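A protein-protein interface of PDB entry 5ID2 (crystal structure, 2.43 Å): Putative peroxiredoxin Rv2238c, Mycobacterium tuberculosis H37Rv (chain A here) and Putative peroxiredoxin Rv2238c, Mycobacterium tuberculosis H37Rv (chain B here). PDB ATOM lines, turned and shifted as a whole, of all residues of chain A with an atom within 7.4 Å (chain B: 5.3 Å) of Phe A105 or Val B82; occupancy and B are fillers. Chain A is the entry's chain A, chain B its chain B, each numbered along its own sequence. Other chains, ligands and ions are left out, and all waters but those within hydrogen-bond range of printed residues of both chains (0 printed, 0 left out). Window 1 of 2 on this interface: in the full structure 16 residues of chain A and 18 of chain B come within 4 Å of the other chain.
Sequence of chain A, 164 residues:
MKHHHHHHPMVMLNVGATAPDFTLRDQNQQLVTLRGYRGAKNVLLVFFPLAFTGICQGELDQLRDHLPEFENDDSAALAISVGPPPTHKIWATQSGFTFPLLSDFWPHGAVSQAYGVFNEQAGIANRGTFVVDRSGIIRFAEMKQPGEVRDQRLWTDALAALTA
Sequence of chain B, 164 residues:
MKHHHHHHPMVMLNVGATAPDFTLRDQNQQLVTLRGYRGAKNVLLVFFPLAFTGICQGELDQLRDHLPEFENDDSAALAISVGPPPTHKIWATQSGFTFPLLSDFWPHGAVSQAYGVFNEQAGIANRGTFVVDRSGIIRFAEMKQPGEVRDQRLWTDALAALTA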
ATOM      1  N   LEU A  24       9.105  27.260   6.926  1.00  0.00           N
ATOM      2  CA  LEU A  24       8.796  26.536   5.692  1.00  0.00           C
ATOM      3  C   LEU A  24       9.933  26.647   4.682  1.00  0.00           C
ATOM      4  O   LEU A  24      10.718  27.589   4.709  1.00  0.00           O
ATOM      5  CB  LEU A  24       7.506  27.077   5.072  1.00  0.00           C
ATOM      6  CG  LEU A  24       6.232  27.006   5.919  1.00  0.00           C
ATOM      7  CD1 LEU A  24       5.100  27.763   5.242  1.00  0.00           C
ATOM      8  CD2 LEU A  24       5.818  25.567   6.189  1.00  0.00           C
ATOM      9  N   ILE A  80       2.298  31.461  -0.175  1.00  0.00           N
ATOM     10  CA  ILE A  80       2.245  30.175   0.506  1.00  0.00           C
ATOM     11  C   ILE A  80       1.182  29.276  -0.111  1.00  0.00           C
ATOM     12  O   ILE A  80       0.035  29.680  -0.282  1.00  0.00           O
ATOM     13  CB  ILE A  80       1.919  30.334   2.007  1.00  0.00           C
ATOM     14  CG1 ILE A  80       2.922  31.277   2.693  1.00  0.00           C
ATOM     15  CG2 ILE A  80       1.925  28.980   2.703  1.00  0.00           C
ATOM     16  CD1 ILE A  80       2.567  31.624   4.133  1.00  0.00           C
ATOM     17  N   SER A  81       1.563  28.033  -0.400  1.00  0.00           N
ATOM     18  CA  SER A  81       0.612  27.037  -0.876  1.00  0.00           C
ATOM     19  C   SER A  81       1.108  25.660  -0.488  1.00  0.00           C
ATOM     20  O   SER A  81       2.246  25.497  -0.040  1.00  0.00           O
ATOM     21  CB  SER A  81       0.388  27.145  -2.386  1.00  0.00           C
ATOM     22  OG  SER A  81       1.145  26.190  -3.096  1.00  0.00           O
ATOM     23  N   VAL A  82       0.267  24.659  -0.711  1.00  0.00           N
ATOM     24  CA  VAL A  82       0.585  23.286  -0.302  1.00  0.00           C
ATOM     25  C   VAL A  82       1.583  22.569  -1.224  1.00  0.00           C
ATOM     26  O   VAL A  82       1.994  21.443  -0.932  1.00  0.00           O
ATOM     27  CB  VAL A  82      -0.682  22.420  -0.155  1.00  0.00           C
ATOM     28  CG1 VAL A  82      -1.633  23.041   0.857  1.00  0.00           C
ATOM     29  CG2 VAL A  82      -1.377  22.205  -1.498  1.00  0.00           C
ATOM     30  N   GLY A  83       1.976  23.210  -2.319  1.00  0.00           N
ATOM     31  CA  GLY A  83       2.937  22.611  -3.242  1.00  0.00           C
ATOM     32  C   GLY A  83       4.330  22.482  -2.650  1.00  0.00           C
ATOM     33  O   GLY A  83       4.739  23.309  -1.834  1.00  0.00           O
ATOM     34  N   PRO A  84       5.070  21.435  -3.058  1.00  0.00           N
ATOM     35  CA  PRO A  84       6.433  21.276  -2.588  1.00  0.00           C
ATOM     36  C   PRO A  84       7.387  22.185  -3.365  1.00  0.00           C
ATOM     37  O   PRO A  84       7.031  22.682  -4.435  1.00  0.00           O
ATOM     38  CB  PRO A  84       6.718  19.809  -2.871  1.00  0.00           C
ATOM     39  CG  PRO A  84       5.935  19.531  -4.106  1.00  0.00           C
ATOM     40  CD  PRO A  84       4.704  20.388  -4.029  1.00  0.00           C
ATOM     41  N   PRO A  85       8.603  22.390  -2.839  1.00  0.00           N
ATOM     42  CA  PRO A  85       9.563  23.298  -3.467  1.00  0.00           C
ATOM     43  C   PRO A  85       9.827  23.094  -4.973  1.00  0.00           C
ATOM     44  O   PRO A  85       9.895  24.070  -5.710  1.00  0.00           O
ATOM     45  CB  PRO A  85      10.831  23.086  -2.631  1.00  0.00           C
ATOM     46  CG  PRO A  85      10.311  22.688  -1.288  1.00  0.00           C
ATOM     47  CD  PRO A  85       9.127  21.824  -1.580  1.00  0.00           C
ATOM     48  N   THR A  87       7.911  22.117  -7.321  1.00  0.00           N
ATOM     49  CA  THR A  87       6.775  22.678  -8.060  1.00  0.00           C
ATOM     50  C   THR A  87       6.875  24.195  -8.112  1.00  0.00           C
ATOM     51  O   THR A  87       6.750  24.784  -9.175  1.00  0.00           O
ATOM     52  CB  THR A  87       5.435  22.255  -7.431  1.00  0.00           C
ATOM     53  OG1 THR A  87       5.240  20.851  -7.652  1.00  0.00           O
ATOM     54  CG2 THR A  87       4.274  23.021  -8.035  1.00  0.00           C
ATOM     55  N   HIS A  88       7.136  24.807  -6.959  1.00  0.00           N
ATOM     56  CA  HIS A  88       7.275  26.249  -6.871  1.00  0.00           C
ATOM     57  C   HIS A  88       8.510  26.779  -7.615  1.00  0.00           C
ATOM     58  O   HIS A  88       8.456  27.852  -8.199  1.00  0.00           O
ATOM     59  CB  HIS A  88       7.302  26.703  -5.417  1.00  0.00           C
ATOM     60  CG  HIS A  88       5.993  26.541  -4.708  1.00  0.00           C
ATOM     61  ND1 HIS A  88       5.897  26.378  -3.340  1.00  0.00           N
ATOM     62  CD2 HIS A  88       4.726  26.508  -5.178  1.00  0.00           C
ATOM     63  CE1 HIS A  88       4.626  26.252  -3.003  1.00  0.00           C
ATOM     64  NE2 HIS A  88       3.895  26.333  -4.099  1.00  0.00           N
ATOM     65  N   LEU A 102       6.502  29.597  -0.492  1.00  0.00           N
ATOM     66  CA  LEU A 102       6.744  28.667   0.606  1.00  0.00           C
ATOM     67  C   LEU A 102       5.825  27.457   0.555  1.00  0.00           C
ATOM     68  O   LEU A 102       4.654  27.567   0.192  1.00  0.00           O
ATOM     69  CB  LEU A 102       6.559  29.368   1.945  1.00  0.00           C
ATOM     70  CG  LEU A 102       7.309  30.688   2.127  1.00  0.00           C
ATOM     71  CD1 LEU A 102       7.086  31.201   3.539  1.00  0.00           C
ATOM     72  CD2 LEU A 102       8.795  30.531   1.835  1.00  0.00           C
ATOM     73  N   SER A 103       6.371  26.308   0.938  1.00  0.00           N
ATOM     74  CA  SER A 103       5.670  25.039   0.841  1.00  0.00           C
ATOM     75  C   SER A 103       5.004  24.648   2.153  1.00  0.00           C
ATOM     76  O   SER A 103       5.674  24.271   3.106  1.00  0.00           O
ATOM     77  CB  SER A 103       6.641  23.934   0.420  1.00  0.00           C
ATOM     78  OG  SER A 103       7.073  24.124  -0.915  1.00  0.00           O
ATOM     79  N   ASP A 104       3.678  24.708   2.172  1.00  0.00           N
ATOM     80  CA  ASP A 104       2.875  24.191   3.273  1.00  0.00           C
ATOM     81  C   ASP A 104       2.490  22.744   2.938  1.00  0.00           C
ATOM     82  O   ASP A 104       1.314  22.396   2.877  1.00  0.00           O
ATOM     83  CB  ASP A 104       1.640  25.075   3.441  1.00  0.00           C
ATOM     84  CG  ASP A 104       0.930  24.864   4.759  1.00  0.00           C
ATOM     85  OD1 ASP A 104       1.530  24.300   5.701  1.00  0.00           O
ATOM     86  OD2 ASP A 104      -0.243  25.278   4.849  1.00  0.00           O
ATOM     87  N   PHE A 105       3.510  21.910   2.735  1.00  0.00           N
ATOM     88  CA  PHE A 105       3.386  20.647   2.022  1.00  0.00           C
ATOM     89  C   PHE A 105       3.274  19.437   2.947  1.00  0.00           C
ATOM     90  O   PHE A 105       2.473  18.532   2.691  1.00  0.00           O
ATOM     91  CB  PHE A 105       4.594  20.494   1.081  1.00  0.00           C
ATOM     92  CG  PHE A 105       4.731  19.133   0.457  1.00  0.00           C
ATOM     93  CD1 PHE A 105       5.677  18.231   0.932  1.00  0.00           C
ATOM     94  CD2 PHE A 105       3.941  18.767  -0.621  1.00  0.00           C
ATOM     95  CE1 PHE A 105       5.817  16.984   0.351  1.00  0.00           C
ATOM     96  CE2 PHE A 105       4.073  17.517  -1.208  1.00  0.00           C
ATOM     97  CZ  PHE A 105       5.013  16.624  -0.722  1.00  0.00           C
ATOM     98  N   TRP A 106       4.103  19.398   3.984  1.00  0.00           N
ATOM     99  CA  TRP A 106       4.148  18.255   4.893  1.00  0.00           C
ATOM    100  C   TRP A 106       4.630  18.679   6.283  1.00  0.00           C
ATOM    101  O   TRP A 106       5.807  18.979   6.453  1.00  0.00           O
ATOM    102  CB  TRP A 106       5.073  17.167   4.329  1.00  0.00           C
ATOM    103  CG  TRP A 106       4.962  15.869   5.062  1.00  0.00           C
ATOM    104  CD1 TRP A 106       5.947  15.241   5.768  1.00  0.00           C
ATOM    105  CD2 TRP A 106       3.796  15.038   5.168  1.00  0.00           C
ATOM    106  NE1 TRP A 106       5.470  14.067   6.309  1.00  0.00           N
ATOM    107  CE2 TRP A 106       4.154  13.918   5.956  1.00  0.00           C
ATOM    108  CE3 TRP A 106       2.495  15.123   4.664  1.00  0.00           C
ATOM    109  CZ2 TRP A 106       3.256  12.899   6.257  1.00  0.00           C
ATOM    110  CZ3 TRP A 106       1.598  14.110   4.970  1.00  0.00           C
ATOM    111  CH2 TRP A 106       1.987  13.007   5.754  1.00  0.00           C
ATOM    112  N   PRO A 107       3.724  18.704   7.283  1.00  0.00           N
ATOM    113  CA  PRO A 107       2.296  18.338   7.235  1.00  0.00           C
ATOM    114  C   PRO A 107       1.461  19.177   6.253  1.00  0.00           C
ATOM    115  O   PRO A 107       1.681  20.381   6.110  1.00  0.00           O
ATOM    116  CB  PRO A 107       1.816  18.549   8.681  1.00  0.00           C
ATOM    117  CG  PRO A 107       2.809  19.469   9.290  1.00  0.00           C
ATOM    118  CD  PRO A 107       4.120  19.184   8.618  1.00  0.00           C
ATOM    119  N   HIS A 108       0.518  18.518   5.586  1.00  0.00           N
ATOM    120  CA  HIS A 108      -0.197  19.090   4.455  1.00  0.00           C
ATOM    121  C   HIS A 108      -1.183  20.157   4.929  1.00  0.00           C
ATOM    122  O   HIS A 108      -2.174  19.843   5.574  1.00  0.00           O
ATOM    123  CB  HIS A 108      -0.917  17.967   3.689  1.00  0.00           C
ATOM    124  CG  HIS A 108      -1.588  18.408   2.421  1.00  0.00           C
ATOM    125  ND1 HIS A 108      -1.430  17.741   1.225  1.00  0.00           N
ATOM    126  CD2 HIS A 108      -2.370  19.480   2.147  1.00  0.00           C
ATOM    127  CE1 HIS A 108      -2.098  18.371   0.279  1.00  0.00           C
ATOM    128  NE2 HIS A 108      -2.677  19.431   0.812  1.00  0.00           N
ATOM    129  N   GLY A 109      -0.914  21.415   4.583  1.00  0.00           N
ATOM    130  CA  GLY A 109      -1.825  22.513   4.882  1.00  0.00           C
ATOM    131  C   GLY A 109      -1.833  22.972   6.332  1.00  0.00           C
ATOM    132  O   GLY A 109      -2.771  23.647   6.760  1.00  0.00           O
ATOM    133  N   ALA A 110      -0.798  22.623   7.092  1.00  0.00           N
ATOM    134  CA  ALA A 110      -0.778  22.916   8.533  1.00  0.00           C
ATOM    135  C   ALA A 110      -0.791  24.413   8.816  1.00  0.00           C
ATOM    136  O   ALA A 110      -1.536  24.885   9.669  1.00  0.00           O
ATOM    137  CB  ALA A 110       0.422  22.263   9.199  1.00  0.00           C
ATOM    138  N   VAL A 111       0.032  25.159   8.094  1.00  0.00           N
ATOM    139  CA  VAL A 111       0.087  26.604   8.283  1.00  0.00           C
ATOM    140  C   VAL A 111      -1.217  27.226   7.811  1.00  0.00           C
ATOM    141  O   VAL A 111      -1.786  28.069   8.505  1.00  0.00           O
ATOM    142  CB  VAL A 111       1.302  27.227   7.571  1.00  0.00           C
ATOM    143  CG1 VAL A 111       1.292  28.736   7.705  1.00  0.00           C
ATOM    144  CG2 VAL A 111       2.589  26.653   8.153  1.00  0.00           C
ATOM    145  N   PHE B  48       6.808   7.767  -7.716  1.00  0.00           N
ATOM    146  CA  PHE B  48       7.921   8.706  -7.737  1.00  0.00           C
ATOM    147  C   PHE B  48       7.673   9.818  -6.734  1.00  0.00           C
ATOM    148  O   PHE B  48       6.518  10.136  -6.435  1.00  0.00           O
ATOM    149  CB  PHE B  48       8.169   9.248  -9.140  1.00  0.00           C
ATOM    150  CG  PHE B  48       7.071  10.116  -9.681  1.00  0.00           C
ATOM    151  CD1 PHE B  48       7.187  11.504  -9.655  1.00  0.00           C
ATOM    152  CD2 PHE B  48       5.952   9.557 -10.263  1.00  0.00           C
ATOM    153  CE1 PHE B  48       6.194  12.313 -10.171  1.00  0.00           C
ATOM    154  CE2 PHE B  48       4.956  10.361 -10.793  1.00  0.00           C
ATOM    155  CZ  PHE B  48       5.082  11.743 -10.755  1.00  0.00           C
ATOM    156  N   PRO B  49       8.758  10.362  -6.155  1.00  0.00           N
ATOM    157  CA  PRO B  49       8.581  11.322  -5.069  1.00  0.00           C
ATOM    158  C   PRO B  49       8.019  12.673  -5.496  1.00  0.00           C
ATOM    159  O   PRO B  49       7.015  13.115  -4.945  1.00  0.00           O
ATOM    160  CB  PRO B  49       9.997  11.456  -4.472  1.00  0.00           C
ATOM    161  CG  PRO B  49      10.917  10.838  -5.442  1.00  0.00           C
ATOM    162  CD  PRO B  49      10.123   9.813  -6.181  1.00  0.00           C
ATOM    163  N   LEU B  50       8.664  13.344  -6.439  1.00  0.00           N
ATOM    164  CA  LEU B  50       8.264  14.707  -6.787  1.00  0.00           C
ATOM    165  C   LEU B  50       8.485  15.026  -8.251  1.00  0.00           C
ATOM    166  O   LEU B  50       9.550  14.745  -8.802  1.00  0.00           O
ATOM    167  CB  LEU B  50       9.050  15.727  -5.952  1.00  0.00           C
ATOM    168  CG  LEU B  50       8.790  15.798  -4.447  1.00  0.00           C
ATOM    169  CD1 LEU B  50       9.813  16.686  -3.758  1.00  0.00           C
ATOM    170  CD2 LEU B  50       7.390  16.303  -4.163  1.00  0.00           C
ATOM    171  N   ILE B  80       2.772   7.356 -10.306  1.00  0.00           N
ATOM    172  CA  ILE B  80       1.978   7.851  -9.182  1.00  0.00           C
ATOM    173  C   ILE B  80       2.820   8.684  -8.232  1.00  0.00           C
ATOM    174  O   ILE B  80       3.908   8.277  -7.824  1.00  0.00           O
ATOM    175  CB  ILE B  80       1.365   6.700  -8.362  1.00  0.00           C
ATOM    176  CG1 ILE B  80       0.543   5.775  -9.262  1.00  0.00           C
ATOM    177  CG2 ILE B  80       0.504   7.257  -7.230  1.00  0.00           C
ATOM    178  CD1 ILE B  80       0.042   4.524  -8.572  1.00  0.00           C
ATOM    179  N   SER B  81       2.300   9.848  -7.864  1.00  0.00           N
ATOM    180  CA  SER B  81       2.989  10.717  -6.930  1.00  0.00           C
ATOM    181  C   SER B  81       1.983  11.635  -6.234  1.00  0.00           C
ATOM    182  O   SER B  81       0.815  11.679  -6.627  1.00  0.00           O
ATOM    183  CB  SER B  81       4.070  11.459  -7.713  1.00  0.00           C
ATOM    184  OG  SER B  81       4.532  12.631  -7.085  1.00  0.00           O
ATOM    185  N   VAL B  82       2.419  12.318  -5.174  1.00  0.00           N
ATOM    186  CA  VAL B  82       1.509  13.117  -4.339  1.00  0.00           C
ATOM    187  C   VAL B  82       1.099  14.449  -4.974  1.00  0.00           C
ATOM    188  O   VAL B  82       0.275  15.173  -4.420  1.00  0.00           O
ATOM    189  CB  VAL B  82       2.078  13.372  -2.917  1.00  0.00           C
ATOM    190  CG1 VAL B  82       2.361  12.055  -2.201  1.00  0.00           C
ATOM    191  CG2 VAL B  82       3.330  14.242  -2.952  1.00  0.00           C
ATOM    192  N   GLY B  83       1.663  14.779  -6.132  1.00  0.00           N
ATOM    193  CA  GLY B  83       1.313  16.014  -6.834  1.00  0.00           C
ATOM    194  C   GLY B  83      -0.109  16.019  -7.372  1.00  0.00           C
ATOM    195  O   GLY B  83      -0.637  14.969  -7.756  1.00  0.00           O
ATOM    196  N   PRO B  84      -0.746  17.203  -7.407  1.00  0.00           N
ATOM    197  CA  PRO B  84      -2.078  17.308  -7.983  1.00  0.00           C
ATOM    198  C   PRO B  84      -2.032  17.367  -9.511  1.00  0.00           C
ATOM    199  O   PRO B  84      -0.960  17.599 -10.085  1.00  0.00           O
ATOM    200  CB  PRO B  84      -2.590  18.627  -7.418  1.00  0.00           C
ATOM    201  CG  PRO B  84      -1.358  19.466  -7.324  1.00  0.00           C
ATOM    202  CD  PRO B  84      -0.226  18.522  -7.005  1.00  0.00           C
ATOM    203  N   HIS B  88       1.144  17.710 -12.618  1.00  0.00           N
ATOM    204  CA  HIS B  88       1.476  16.622 -13.523  1.00  0.00           C
ATOM    205  C   HIS B  88       1.205  16.973 -14.985  1.00  0.00           C
ATOM    206  O   HIS B  88       1.938  16.533 -15.875  1.00  0.00           O
ATOM    207  CB  HIS B  88       0.728  15.345 -13.128  1.00  0.00           C
ATOM    208  CG  HIS B  88       1.201  14.744 -11.839  1.00  0.00           C
ATOM    209  ND1 HIS B  88       0.391  13.974 -11.032  1.00  0.00           N
ATOM    210  CD2 HIS B  88       2.397  14.813 -11.211  1.00  0.00           C
ATOM    211  CE1 HIS B  88       1.075  13.577  -9.974  1.00  0.00           C
ATOM    212  NE2 HIS B  88       2.293  14.081 -10.054  1.00  0.00           N
ATOM    213  N   SER B 103      -2.530  11.317  -9.354  1.00  0.00           N
ATOM    214  CA  SER B 103      -2.379  12.167  -8.161  1.00  0.00           C
ATOM    215  C   SER B 103      -2.804  11.479  -6.878  1.00  0.00           C
ATOM    216  O   SER B 103      -3.995  11.253  -6.654  1.00  0.00           O
ATOM    217  CB  SER B 103      -3.194  13.448  -8.317  1.00  0.00           C
ATOM    218  OG  SER B 103      -2.644  14.263  -9.338  1.00  0.00           O
ATOM    219  N   ASP B 104      -1.820  11.154  -6.043  1.00  0.00           N
ATOM    220  CA  ASP B 104      -2.058  10.642  -4.707  1.00  0.00           C
ATOM    221  C   ASP B 104      -2.011  11.840  -3.747  1.00  0.00           C
ATOM    222  O   ASP B 104      -1.220  11.871  -2.799  1.00  0.00           O
ATOM    223  CB  ASP B 104      -0.977   9.615  -4.362  1.00  0.00           C
ATOM    224  CG  ASP B 104      -1.324   8.775  -3.147  1.00  0.00           C
ATOM    225  OD1 ASP B 104      -2.515   8.719  -2.757  1.00  0.00           O
ATOM    226  OD2 ASP B 104      -0.389   8.157  -2.593  1.00  0.00           O
ATOM    227  N   PHE B 105      -2.906  12.798  -3.987  1.00  0.00           N
ATOM    228  CA  PHE B 105      -2.773  14.167  -3.479  1.00  0.00           C
ATOM    229  C   PHE B 105      -3.600  14.468  -2.237  1.00  0.00           C
ATOM    230  O   PHE B 105      -3.110  15.099  -1.298  1.00  0.00           O
ATOM    231  CB  PHE B 105      -3.151  15.142  -4.599  1.00  0.00           C
ATOM    232  CG  PHE B 105      -3.292  16.573  -4.153  1.00  0.00           C
ATOM    233  CD1 PHE B 105      -4.545  17.140  -3.971  1.00  0.00           C
ATOM    234  CD2 PHE B 105      -2.167  17.362  -3.936  1.00  0.00           C
ATOM    235  CE1 PHE B 105      -4.675  18.464  -3.565  1.00  0.00           C
ATOM    236  CE2 PHE B 105      -2.288  18.681  -3.536  1.00  0.00           C
ATOM    237  CZ  PHE B 105      -3.544  19.234  -3.348  1.00  0.00           C
ATOM    238  N   HIS B 108      -3.424  12.858   1.344  1.00  0.00           N
ATOM    239  CA  HIS B 108      -2.032  12.995   0.934  1.00  0.00           C
ATOM    240  C   HIS B 108      -1.281  11.685   1.146  1.00  0.00           C
ATOM    241  O   HIS B 108      -1.064  11.268   2.282  1.00  0.00           O
ATOM    242  CB  HIS B 108      -1.390  14.135   1.742  1.00  0.00           C
ATOM    243  CG  HIS B 108       0.014  14.461   1.349  1.00  0.00           C
ATOM    244  ND1 HIS B 108       0.440  15.749   1.125  1.00  0.00           N
ATOM    245  CD2 HIS B 108       1.077  13.665   1.085  1.00  0.00           C
ATOM    246  CE1 HIS B 108       1.714  15.735   0.781  1.00  0.00           C
ATOM    247  NE2 HIS B 108       2.126  14.482   0.753  1.00  0.00           N
ATOM    248  N   GLY B 109      -0.897  11.037   0.047  1.00  0.00           N
ATOM    249  CA  GLY B 109      -0.090   9.828   0.112  1.00  0.00           C
ATOM    250  C   GLY B 109      -0.830   8.571   0.536  1.00  0.00           C
ATOM    251  O   GLY B 109      -0.197   7.586   0.923  1.00  0.00           O
ATOM    252  N   SER B 112       0.070   5.574  -1.696  1.00  0.00           N
ATOM    253  CA  SER B 112       1.459   5.253  -1.368  1.00  0.00           C
ATOM    254  C   SER B 112       1.582   4.500  -0.039  1.00  0.00           C
ATOM    255  O   SER B 112       2.362   3.548   0.076  1.00  0.00           O
ATOM    256  CB  SER B 112       2.314   6.520  -1.338  1.00  0.00           C
ATOM    257  OG  SER B 112       2.273   7.179  -2.596  1.00  0.00           O
ATOM    258  N   PHE B 118       5.350   4.908   1.275  1.00  0.00           N
ATOM    259  CA  PHE B 118       5.295   6.308   1.635  1.00  0.00           C
ATOM    260  C   PHE B 118       6.413   6.641   2.613  1.00  0.00           C
ATOM    261  O   PHE B 118       6.646   5.913   3.569  1.00  0.00           O
ATOM    262  CB  PHE B 118       3.942   6.632   2.251  1.00  0.00           C
ATOM    263  CG  PHE B 118       3.701   8.100   2.443  1.00  0.00           C
ATOM    264  CD1 PHE B 118       3.670   8.958   1.349  1.00  0.00           C
ATOM    265  CD2 PHE B 118       3.489   8.618   3.713  1.00  0.00           C
ATOM    266  CE1 PHE B 118       3.434  10.304   1.516  1.00  0.00           C
ATOM    267  CE2 PHE B 118       3.253   9.966   3.887  1.00  0.00           C
ATOM    268  CZ  PHE B 118       3.219  10.812   2.786  1.00  0.00           C
ATOM    269  N   ALA B 122       9.447  12.845   4.945  1.00  0.00           N
ATOM    270  CA  ALA B 122       9.407  13.849   3.877  1.00  0.00           C
ATOM    271  C   ALA B 122       8.010  14.098   3.274  1.00  0.00           C
ATOM    272  O   ALA B 122       7.780  15.131   2.642  1.00  0.00           O
ATOM    273  CB  ALA B 122      10.375  13.455   2.778  1.00  0.00           C
ATOM    274  N   GLY B 123       7.074  13.175   3.481  1.00  0.00           N
ATOM    275  CA  GLY B 123       5.716  13.315   2.930  1.00  0.00           C
ATOM    276  C   GLY B 123       5.641  13.088   1.433  1.00  0.00           C
ATOM    277  O   GLY B 123       4.878  13.743   0.735  1.00  0.00           O
ATOM    278  N   ILE B 124       6.449  12.164   0.937  1.00  0.00           N
ATOM    279  CA  ILE B 124       6.475  11.832  -0.481  1.00  0.00           C
ATOM    280  C   ILE B 124       6.557  10.324  -0.640  1.00  0.00           C
ATOM    281  O   ILE B 124       6.950   9.620   0.288  1.00  0.00           O
ATOM    282  CB  ILE B 124       7.683  12.474  -1.187  1.00  0.00           C
ATOM    283  CG1 ILE B 124       8.991  12.061  -0.494  1.00  0.00           C
ATOM    284  CG2 ILE B 124       7.514  13.983  -1.220  1.00  0.00           C
ATOM    285  CD1 ILE B 124      10.239  12.702  -1.058  1.00  0.00           C
ATOM    286  N   ALA B 125       6.180   9.823  -1.807  1.00  0.00           N
ATOM    287  CA  ALA B 125       6.387   8.414  -2.102  1.00  0.00           C
ATOM    288  C   ALA B 125       7.878   8.173  -2.328  1.00  0.00           C
ATOM    289  O   ALA B 125       8.554   8.985  -2.953  1.00  0.00           O
ATOM    290  CB  ALA B 125       5.592   8.000  -3.324  1.00  0.00           C
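A ring nitrogen (ND1) of His B108 lies within hydrogen-bond range of a ring nitrogen (ND1) of His A108, 2.7 Å away.
The indole nitrogen (NE1) of Trp A106 lies close to the backbone NH (N) of Gly B123 (3.4 Å).
A ring nitrogen (NE2) of His B108 is in hydrogen-bond range of the backbone carbonyl oxygen of Gly B123, 2.8 Å away.
O of Ser B112 is in hydrogen-bond range of N of Phe B118 (3.5 Å).
Among the printed residues, merely in contact across the chains: Phe A105 with Gly B123 (3.2 Å), Trp A106 with Ala B122 (3.4 Å), Phe A105 with His B108 (3.5 Å), Phe A105 with Ala B122 (3.5 Å), Pro A84 with Leu B50 (3.5 Å), Phe A105 with Ile B124 (3.7 Å), Phe A105 with Val B82 (3.7 Å), His A108 with Phe B105 (3.8 Å), Trp A106 with Phe B118 (3.8 Å) and Trp A106 with His B108 (3.9 Å).
Of chain A, only Phe A105 (3.7 Å) comes within 4 Å of Val B82.
No residue of chain A comes within 4 Å of Gly B83.
Of the printed residues of chain A, Ala B122 touches Phe A105 (3.5 Å) and Trp A106 (3.4 Å).
Of the printed residues of chain A, Gly B123 touches Phe A105 (3.2 Å) and Trp A106 (3.3 Å).
Printed residues of chain A within 4 Å of Ile B124: Phe A105 (3.7 Å).
The nearest residue of chain A that does not touch Val B82 is Pro A84 (6.0 Å).
The nearest printed residue of chain A that does not touch Phe B118 is Phe A105 (6.9 Å).
Of the 19 printed residues of chain A, 4 touch a printed residue of chain B.
Printed residues of chain A that touch a printed residue of chain B: Pro A84, Phe A105, Trp A106 and His A108.
Of the 20 printed residues of chain B, 8 touch a printed residue of chain A.
Hydrophobic or aromatic side chains of chain B within 4 Å of the printed part of chain A: Leu B50, Val B82, Phe B105, His B108, Phe B118 and Ile B124.
Among the printed residues, 12 pairs touch across the chains.
Among the printed residues, no Asp or Glu carboxylate lies within 4 Å of a Lys or Arg side-chain nitrogen of the other chain.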
